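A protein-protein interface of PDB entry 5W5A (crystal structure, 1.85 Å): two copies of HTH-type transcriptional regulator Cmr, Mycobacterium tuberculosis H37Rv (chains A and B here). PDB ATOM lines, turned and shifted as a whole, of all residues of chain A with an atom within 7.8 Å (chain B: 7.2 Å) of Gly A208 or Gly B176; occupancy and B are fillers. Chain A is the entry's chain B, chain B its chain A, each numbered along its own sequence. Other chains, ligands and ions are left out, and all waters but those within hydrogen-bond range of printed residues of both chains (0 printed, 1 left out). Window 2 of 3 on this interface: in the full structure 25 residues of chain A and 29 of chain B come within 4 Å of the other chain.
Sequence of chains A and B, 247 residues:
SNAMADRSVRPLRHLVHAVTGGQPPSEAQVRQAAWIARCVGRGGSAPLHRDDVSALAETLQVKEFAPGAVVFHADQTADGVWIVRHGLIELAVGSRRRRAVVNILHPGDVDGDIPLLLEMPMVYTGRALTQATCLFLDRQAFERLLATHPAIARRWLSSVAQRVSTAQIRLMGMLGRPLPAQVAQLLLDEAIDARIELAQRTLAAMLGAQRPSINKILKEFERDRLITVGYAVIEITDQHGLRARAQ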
ATOM      1  N   GLU A  27     -18.066  -7.156  30.269  1.00  0.00           N
ATOM      2  CA  GLU A  27     -18.579  -8.079  29.252  1.00  0.00           C
ATOM      3  C   GLU A  27     -17.573  -9.167  28.969  1.00  0.00           C
ATOM      4  O   GLU A  27     -17.920 -10.349  28.855  1.00  0.00           O
ATOM      5  CB  GLU A  27     -18.925  -7.369  27.938  1.00  0.00           C
ATOM      6  CG  GLU A  27     -19.443  -8.379  26.913  1.00  0.00           C
ATOM      7  CD  GLU A  27     -19.670  -7.823  25.523  1.00  0.00           C
ATOM      8  OE1 GLU A  27     -19.161  -6.718  25.239  1.00  0.00           O
ATOM      9  OE2 GLU A  27     -20.371  -8.495  24.721  1.00  0.00           O
ATOM     10  N   ARG A  31     -18.162 -13.162  29.461  1.00  0.00           N
ATOM     11  CA  ARG A  31     -18.048 -14.067  28.328  1.00  0.00           C
ATOM     12  C   ARG A  31     -17.031 -15.167  28.615  1.00  0.00           C
ATOM     13  O   ARG A  31     -17.295 -16.349  28.398  1.00  0.00           O
ATOM     14  CB  ARG A  31     -17.634 -13.316  27.066  1.00  0.00           C
ATOM     15  CG  ARG A  31     -17.169 -14.244  25.954  1.00  0.00           C
ATOM     16  CD  ARG A  31     -17.074 -13.519  24.626  1.00  0.00           C
ATOM     17  NE  ARG A  31     -16.309 -12.298  24.748  1.00  0.00           N
ATOM     18  CZ  ARG A  31     -16.838 -11.077  24.811  1.00  0.00           C
ATOM     19  NH1 ARG A  31     -18.165 -10.868  24.749  1.00  0.00           N
ATOM     20  NH2 ARG A  31     -16.017 -10.063  24.932  1.00  0.00           N
ATOM     21  N   TRP A  35     -18.083 -19.256  29.046  1.00  0.00           N
ATOM     22  CA  TRP A  35     -17.695 -20.290  28.092  1.00  0.00           C
ATOM     23  C   TRP A  35     -16.749 -21.282  28.766  1.00  0.00           C
ATOM     24  O   TRP A  35     -16.810 -22.470  28.502  1.00  0.00           O
ATOM     25  CB  TRP A  35     -17.085 -19.695  26.824  1.00  0.00           C
ATOM     26  CG  TRP A  35     -18.177 -19.252  25.864  1.00  0.00           C
ATOM     27  CD1 TRP A  35     -18.478 -17.964  25.501  1.00  0.00           C
ATOM     28  CD2 TRP A  35     -19.136 -20.091  25.201  1.00  0.00           C
ATOM     29  NE1 TRP A  35     -19.553 -17.962  24.644  1.00  0.00           N
ATOM     30  CE2 TRP A  35     -19.972 -19.249  24.438  1.00  0.00           C
ATOM     31  CE3 TRP A  35     -19.381 -21.474  25.191  1.00  0.00           C
ATOM     32  CZ2 TRP A  35     -21.027 -19.744  23.666  1.00  0.00           C
ATOM     33  CZ3 TRP A  35     -20.419 -21.966  24.401  1.00  0.00           C
ATOM     34  CH2 TRP A  35     -21.228 -21.106  23.659  1.00  0.00           C
ATOM     35  N   LEU A 179     -28.314 -13.638  14.218  1.00  0.00           N
ATOM     36  CA  LEU A 179     -28.381 -13.579  15.678  1.00  0.00           C
ATOM     37  C   LEU A 179     -29.639 -14.237  16.276  1.00  0.00           C
ATOM     38  O   LEU A 179     -29.526 -14.952  17.267  1.00  0.00           O
ATOM     39  CB  LEU A 179     -28.262 -12.123  16.153  1.00  0.00           C
ATOM     40  CG  LEU A 179     -28.049 -11.880  17.654  1.00  0.00           C
ATOM     41  CD1 LEU A 179     -26.858 -12.691  18.240  1.00  0.00           C
ATOM     42  CD2 LEU A 179     -27.894 -10.390  17.934  1.00  0.00           C
ATOM     43  N   GLN A 182     -29.056 -17.764  16.568  1.00  0.00           N
ATOM     44  CA  GLN A 182     -28.071 -18.036  17.600  1.00  0.00           C
ATOM     45  C   GLN A 182     -28.685 -17.978  18.977  1.00  0.00           C
ATOM     46  O   GLN A 182     -28.343 -18.765  19.855  1.00  0.00           O
ATOM     47  CB  GLN A 182     -26.939 -17.038  17.540  1.00  0.00           C
ATOM     48  CG  GLN A 182     -26.102 -17.104  16.290  1.00  0.00           C
ATOM     49  CD  GLN A 182     -24.955 -16.158  16.415  1.00  0.00           C
ATOM     50  OE1 GLN A 182     -24.265 -16.158  17.432  1.00  0.00           O
ATOM     51  NE2 GLN A 182     -24.754 -15.321  15.409  1.00  0.00           N
ATOM     52  N   THR A 202     -25.888 -11.921  30.454  1.00  0.00           N
ATOM     53  CA  THR A 202     -24.976 -13.050  30.327  1.00  0.00           C
ATOM     54  C   THR A 202     -25.162 -13.713  28.961  1.00  0.00           C
ATOM     55  O   THR A 202     -24.188 -14.057  28.298  1.00  0.00           O
ATOM     56  CB  THR A 202     -25.197 -14.053  31.474  1.00  0.00           C
ATOM     57  OG1 THR A 202     -24.933 -13.392  32.719  1.00  0.00           O
ATOM     58  CG2 THR A 202     -24.255 -15.304  31.350  1.00  0.00           C
ATOM     59  N   LEU A 203     -26.400 -13.868  28.515  1.00  0.00           N
ATOM     60  CA  LEU A 203     -26.644 -14.408  27.164  1.00  0.00           C
ATOM     61  C   LEU A 203     -25.974 -13.525  26.100  1.00  0.00           C
ATOM     62  O   LEU A 203     -25.274 -14.015  25.211  1.00  0.00           O
ATOM     63  CB  LEU A 203     -28.144 -14.497  26.859  1.00  0.00           C
ATOM     64  CG  LEU A 203     -28.996 -15.377  27.758  1.00  0.00           C
ATOM     65  CD1 LEU A 203     -30.477 -15.173  27.431  1.00  0.00           C
ATOM     66  CD2 LEU A 203     -28.565 -16.829  27.596  1.00  0.00           C
ATOM     67  N   ALA A 204     -26.178 -12.221  26.216  1.00  0.00           N
ATOM     68  CA  ALA A 204     -25.555 -11.259  25.294  1.00  0.00           C
ATOM     69  C   ALA A 204     -24.027 -11.402  25.283  1.00  0.00           C
ATOM     70  O   ALA A 204     -23.408 -11.434  24.213  1.00  0.00           O
ATOM     71  CB  ALA A 204     -25.968  -9.842  25.678  1.00  0.00           C
ATOM     72  N   ALA A 205     -23.426 -11.513  26.469  1.00  0.00           N
ATOM     73  CA  ALA A 205     -21.979 -11.653  26.598  1.00  0.00           C
ATOM     74  C   ALA A 205     -21.521 -12.939  25.920  1.00  0.00           C
ATOM     75  O   ALA A 205     -20.527 -12.939  25.219  1.00  0.00           O
ATOM     76  CB  ALA A 205     -21.562 -11.644  28.063  1.00  0.00           C
ATOM     77  N   MET A 206     -22.251 -14.038  26.105  1.00  0.00           N
ATOM     78  CA  MET A 206     -21.838 -15.308  25.474  1.00  0.00           C
ATOM     79  C   MET A 206     -21.881 -15.266  23.953  1.00  0.00           C
ATOM     80  O   MET A 206     -21.168 -16.023  23.298  1.00  0.00           O
ATOM     81  CB  MET A 206     -22.720 -16.453  25.966  1.00  0.00           C
ATOM     82  CG  MET A 206     -22.526 -16.712  27.404  1.00  0.00           C
ATOM     83  SD  MET A 206     -23.718 -18.163  27.959  1.00  0.00           S
ATOM     84  CE  MET A 206     -22.715 -19.757  27.213  1.00  0.00           C
ATOM     85  N   LEU A 207     -22.700 -14.376  23.387  1.00  0.00           N
ATOM     86  CA  LEU A 207     -22.842 -14.338  21.933  1.00  0.00           C
ATOM     87  C   LEU A 207     -22.064 -13.187  21.330  1.00  0.00           C
ATOM     88  O   LEU A 207     -22.068 -13.002  20.117  1.00  0.00           O
ATOM     89  CB  LEU A 207     -24.319 -14.228  21.525  1.00  0.00           C
ATOM     90  CG  LEU A 207     -25.204 -15.425  21.879  1.00  0.00           C
ATOM     91  CD1 LEU A 207     -26.615 -15.157  21.463  1.00  0.00           C
ATOM     92  CD2 LEU A 207     -24.674 -16.745  21.240  1.00  0.00           C
ATOM     93  N   GLY A 208     -21.408 -12.394  22.169  1.00  0.00           N
ATOM     94  CA  GLY A 208     -20.736 -11.213  21.684  1.00  0.00           C
ATOM     95  C   GLY A 208     -21.730 -10.219  21.073  1.00  0.00           C
ATOM     96  O   GLY A 208     -21.421  -9.519  20.111  1.00  0.00           O
ATOM     97  N   ALA A 209     -22.932 -10.177  21.626  1.00  0.00           N
ATOM     98  CA  ALA A 209     -24.003  -9.346  21.078  1.00  0.00           C
ATOM     99  C   ALA A 209     -24.310  -8.128  21.942  1.00  0.00           C
ATOM    100  O   ALA A 209     -24.171  -8.171  23.151  1.00  0.00           O
ATOM    101  CB  ALA A 209     -25.268 -10.191  20.899  1.00  0.00           C
ATOM    102  N   GLN A 210     -24.724  -7.049  21.296  1.00  0.00           N
ATOM    103  CA  GLN A 210     -25.247  -5.865  21.978  1.00  0.00           C
ATOM    104  C   GLN A 210     -26.508  -6.201  22.774  1.00  0.00           C
ATOM    105  O   GLN A 210     -27.376  -6.934  22.303  1.00  0.00           O
ATOM    106  CB  GLN A 210     -25.542  -4.788  20.956  1.00  0.00           C
ATOM    107  CG  GLN A 210     -24.309  -4.298  20.228  1.00  0.00           C
ATOM    108  CD  GLN A 210     -23.473  -3.369  21.080  1.00  0.00           C
ATOM    109  OE1 GLN A 210     -22.694  -3.814  21.927  1.00  0.00           O
ATOM    110  NE2 GLN A 210     -23.637  -2.067  20.868  1.00  0.00           N
ATOM    111  N   ARG A 211     -26.609  -5.671  23.980  1.00  0.00           N
ATOM    112  CA  ARG A 211     -27.729  -5.999  24.849  1.00  0.00           C
ATOM    113  C   ARG A 211     -29.119  -5.574  24.315  1.00  0.00           C
ATOM    114  O   ARG A 211     -30.069  -6.344  24.439  1.00  0.00           O
ATOM    115  CB  ARG A 211     -27.460  -5.415  26.239  1.00  0.00           C
ATOM    116  CG  ARG A 211     -26.325  -6.186  26.964  1.00  0.00           C
ATOM    117  CD  ARG A 211     -25.886  -5.459  28.227  1.00  0.00           C
ATOM    118  NE  ARG A 211     -26.953  -5.447  29.204  1.00  0.00           N
ATOM    119  CZ  ARG A 211     -26.915  -4.736  30.323  1.00  0.00           C
ATOM    120  NH1 ARG A 211     -25.851  -3.991  30.585  1.00  0.00           N
ATOM    121  NH2 ARG A 211     -27.936  -4.773  31.171  1.00  0.00           N
ATOM    122  N   ILE A 214     -30.295  -8.260  21.813  1.00  0.00           N
ATOM    123  CA  ILE A 214     -30.735  -9.487  22.473  1.00  0.00           C
ATOM    124  C   ILE A 214     -32.147  -9.299  23.058  1.00  0.00           C
ATOM    125  O   ILE A 214     -33.040 -10.114  22.841  1.00  0.00           O
ATOM    126  CB  ILE A 214     -29.730  -9.904  23.577  1.00  0.00           C
ATOM    127  CG1 ILE A 214     -28.394 -10.315  22.945  1.00  0.00           C
ATOM    128  CG2 ILE A 214     -30.286 -11.027  24.448  1.00  0.00           C
ATOM    129  CD1 ILE A 214     -28.499 -11.421  21.896  1.00  0.00           C
ATOM    130  N   LEU B 171     -11.809 -18.894  19.327  1.00  0.00           N
ATOM    131  CA  LEU B 171     -13.236 -18.663  18.990  1.00  0.00           C
ATOM    132  C   LEU B 171     -13.890 -17.648  19.927  1.00  0.00           C
ATOM    133  O   LEU B 171     -14.635 -16.769  19.471  1.00  0.00           O
ATOM    134  CB  LEU B 171     -14.027 -19.970  19.020  1.00  0.00           C
ATOM    135  CG  LEU B 171     -13.673 -20.904  17.853  1.00  0.00           C
ATOM    136  CD1 LEU B 171     -14.051 -22.360  18.167  1.00  0.00           C
ATOM    137  CD2 LEU B 171     -14.359 -20.398  16.587  1.00  0.00           C
ATOM    138  N   MET B 172     -13.628 -17.770  21.219  1.00  0.00           N
ATOM    139  CA  MET B 172     -14.154 -16.807  22.183  1.00  0.00           C
ATOM    140  C   MET B 172     -13.677 -15.392  21.872  1.00  0.00           C
ATOM    141  O   MET B 172     -14.435 -14.408  22.052  1.00  0.00           O
ATOM    142  CB  MET B 172     -13.743 -17.183  23.601  1.00  0.00           C
ATOM    143  CG  MET B 172     -14.418 -18.419  24.135  1.00  0.00           C
ATOM    144  SD  MET B 172     -13.625 -18.939  25.847  1.00  0.00           S
ATOM    145  CE  MET B 172     -13.304 -17.191  26.567  1.00  0.00           C
ATOM    146  N   GLY B 173     -12.427 -15.282  21.439  1.00  0.00           N
ATOM    147  CA  GLY B 173     -11.809 -13.984  21.264  1.00  0.00           C
ATOM    148  C   GLY B 173     -12.296 -13.283  20.012  1.00  0.00           C
ATOM    149  O   GLY B 173     -11.988 -12.115  19.799  1.00  0.00           O
ATOM    150  N   MET B 174     -13.037 -14.002  19.172  1.00  0.00           N
ATOM    151  CA  MET B 174     -13.652 -13.426  17.968  1.00  0.00           C
ATOM    152  C   MET B 174     -14.992 -12.757  18.277  1.00  0.00           C
ATOM    153  O   MET B 174     -15.439 -11.875  17.547  1.00  0.00           O
ATOM    154  CB  MET B 174     -13.856 -14.517  16.900  1.00  0.00           C
ATOM    155  CG  MET B 174     -12.592 -14.869  16.165  1.00  0.00           C
ATOM    156  SD  MET B 174     -12.753 -16.716  15.460  1.00  0.00           S
ATOM    157  CE  MET B 174     -14.434 -16.615  14.507  1.00  0.00           C
ATOM    158  N   LEU B 175     -15.604 -13.157  19.377  1.00  0.00           N
ATOM    159  CA  LEU B 175     -16.983 -12.784  19.667  1.00  0.00           C
ATOM    160  C   LEU B 175     -17.127 -11.282  19.804  1.00  0.00           C
ATOM    161  O   LEU B 175     -16.460 -10.659  20.635  1.00  0.00           O
ATOM    162  CB  LEU B 175     -17.472 -13.465  20.950  1.00  0.00           C
ATOM    163  CG  LEU B 175     -17.637 -14.980  20.761  1.00  0.00           C
ATOM    164  CD1 LEU B 175     -18.068 -15.652  22.056  1.00  0.00           C
ATOM    165  CD2 LEU B 175     -18.672 -15.260  19.711  1.00  0.00           C
ATOM    166  N   GLY B 176     -17.974 -10.717  18.958  1.00  0.00           N
ATOM    167  CA  GLY B 176     -18.352  -9.326  19.095  1.00  0.00           C
ATOM    168  C   GLY B 176     -17.341  -8.335  18.536  1.00  0.00           C
ATOM    169  O   GLY B 176     -17.511  -7.118  18.676  1.00  0.00           O
ATOM    170  N   ARG B 177     -16.293  -8.841  17.903  1.00  0.00           N
ATOM    171  CA  ARG B 177     -15.254  -7.974  17.360  1.00  0.00           C
ATOM    172  C   ARG B 177     -15.569  -7.611  15.914  1.00  0.00           C
ATOM    173  O   ARG B 177     -16.195  -8.392  15.199  1.00  0.00           O
ATOM    174  CB  ARG B 177     -13.882  -8.672  17.473  1.00  0.00           C
ATOM    175  CG  ARG B 177     -13.617  -9.129  18.896  1.00  0.00           C
ATOM    176  CD  ARG B 177     -12.210  -8.938  19.333  1.00  0.00           C
ATOM    177  NE  ARG B 177     -11.262  -9.531  18.391  1.00  0.00           N
ATOM    178  CZ  ARG B 177     -10.182  -8.890  17.964  1.00  0.00           C
ATOM    179  NH1 ARG B 177      -9.952  -7.659  18.405  1.00  0.00           N
ATOM    180  NH2 ARG B 177      -9.334  -9.466  17.127  1.00  0.00           N
ATOM    181  N   PRO B 178     -15.125  -6.423  15.470  1.00  0.00           N
ATOM    182  CA  PRO B 178     -15.340  -6.062  14.068  1.00  0.00           C
ATOM    183  C   PRO B 178     -14.614  -7.017  13.132  1.00  0.00           C
ATOM    184  O   PRO B 178     -13.561  -7.568  13.515  1.00  0.00           O
ATOM    185  CB  PRO B 178     -14.761  -4.638  13.966  1.00  0.00           C
ATOM    186  CG  PRO B 178     -14.815  -4.080  15.396  1.00  0.00           C
ATOM    187  CD  PRO B 178     -14.581  -5.318  16.278  1.00  0.00           C
ATOM    188  N   LEU B 179     -15.151  -7.227  11.929  1.00  0.00           N
ATOM    189  CA  LEU B 179     -14.570  -8.186  10.992  1.00  0.00           C
ATOM    190  C   LEU B 179     -13.121  -7.880  10.591  1.00  0.00           C
ATOM    191  O   LEU B 179     -12.321  -8.811  10.469  1.00  0.00           O
ATOM    192  CB  LEU B 179     -15.439  -8.303   9.738  1.00  0.00           C
ATOM    193  CG  LEU B 179     -15.044  -9.438   8.782  1.00  0.00           C
ATOM    194  CD1 LEU B 179     -14.998 -10.809   9.515  1.00  0.00           C
ATOM    195  CD2 LEU B 179     -16.007  -9.497   7.605  1.00  0.00           C
ATOM    196  N   GLN B 182     -10.907  -9.202  13.251  1.00  0.00           N
ATOM    197  CA  GLN B 182     -10.930 -10.663  13.199  1.00  0.00           C
ATOM    198  C   GLN B 182     -10.031 -11.232  12.101  1.00  0.00           C
ATOM    199  O   GLN B 182      -9.407 -12.265  12.289  1.00  0.00           O
ATOM    200  CB  GLN B 182     -12.335 -11.177  12.962  1.00  0.00           C
ATOM    201  CG  GLN B 182     -13.309 -10.970  14.127  1.00  0.00           C
ATOM    202  CD  GLN B 182     -14.563 -11.780  13.902  1.00  0.00           C
ATOM    203  OE1 GLN B 182     -14.513 -13.004  13.797  1.00  0.00           O
ATOM    204  NE2 GLN B 182     -15.670 -11.122  13.792  1.00  0.00           N
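The guanidinium group (NH1) of Arg A31 lies within salt-bridge range of the side-chain carboxylate (OE2) of Glu A27, 3.2 Å away.
O of Ala A205 sits at hydrogen-bond distance from NH1 of Arg A31.
NE1 of Trp A35 is in hydrogen-bond range of O of Met A206.
Among the printed residues, pairs that only touch across the chains: Gly A208 with Gly B176, Met A206 with Leu B175, Arg A31 with Leu B175, Trp A35 with Met B172, Trp A35 with Leu B175 and Arg A31 with Met B172.
Gly A208 touches just one residue of chain B: Gly B176 (3.2 Å).
Of chain A, only Gly A208 (3.2 Å) comes within 4 Å of Gly B176.
Of the printed residues of chain A, Met B172 touches Arg A31 (3.8 Å) and Trp A35 (3.7 Å).
Printed residues of chain B within 4 Å of Trp A35: Met B172 (3.7 Å) and Leu B175 (3.8 Å).
Ala A204 touches none of the printed residues of chain B.
The nearest residue of chain B that does not touch Gly A208 is Leu B175 (4.03 Å).
Hydrophobic or aromatic side chains of chain A within 4 Å of the printed part of chain B: Trp A35.
Among the printed residues, 6 pairs touch across the chains.
2 positions are printed for both chains.
Of the 6 pairs that touch across the chains among the printed residues, none has its exchanged pair printed and touching as well.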
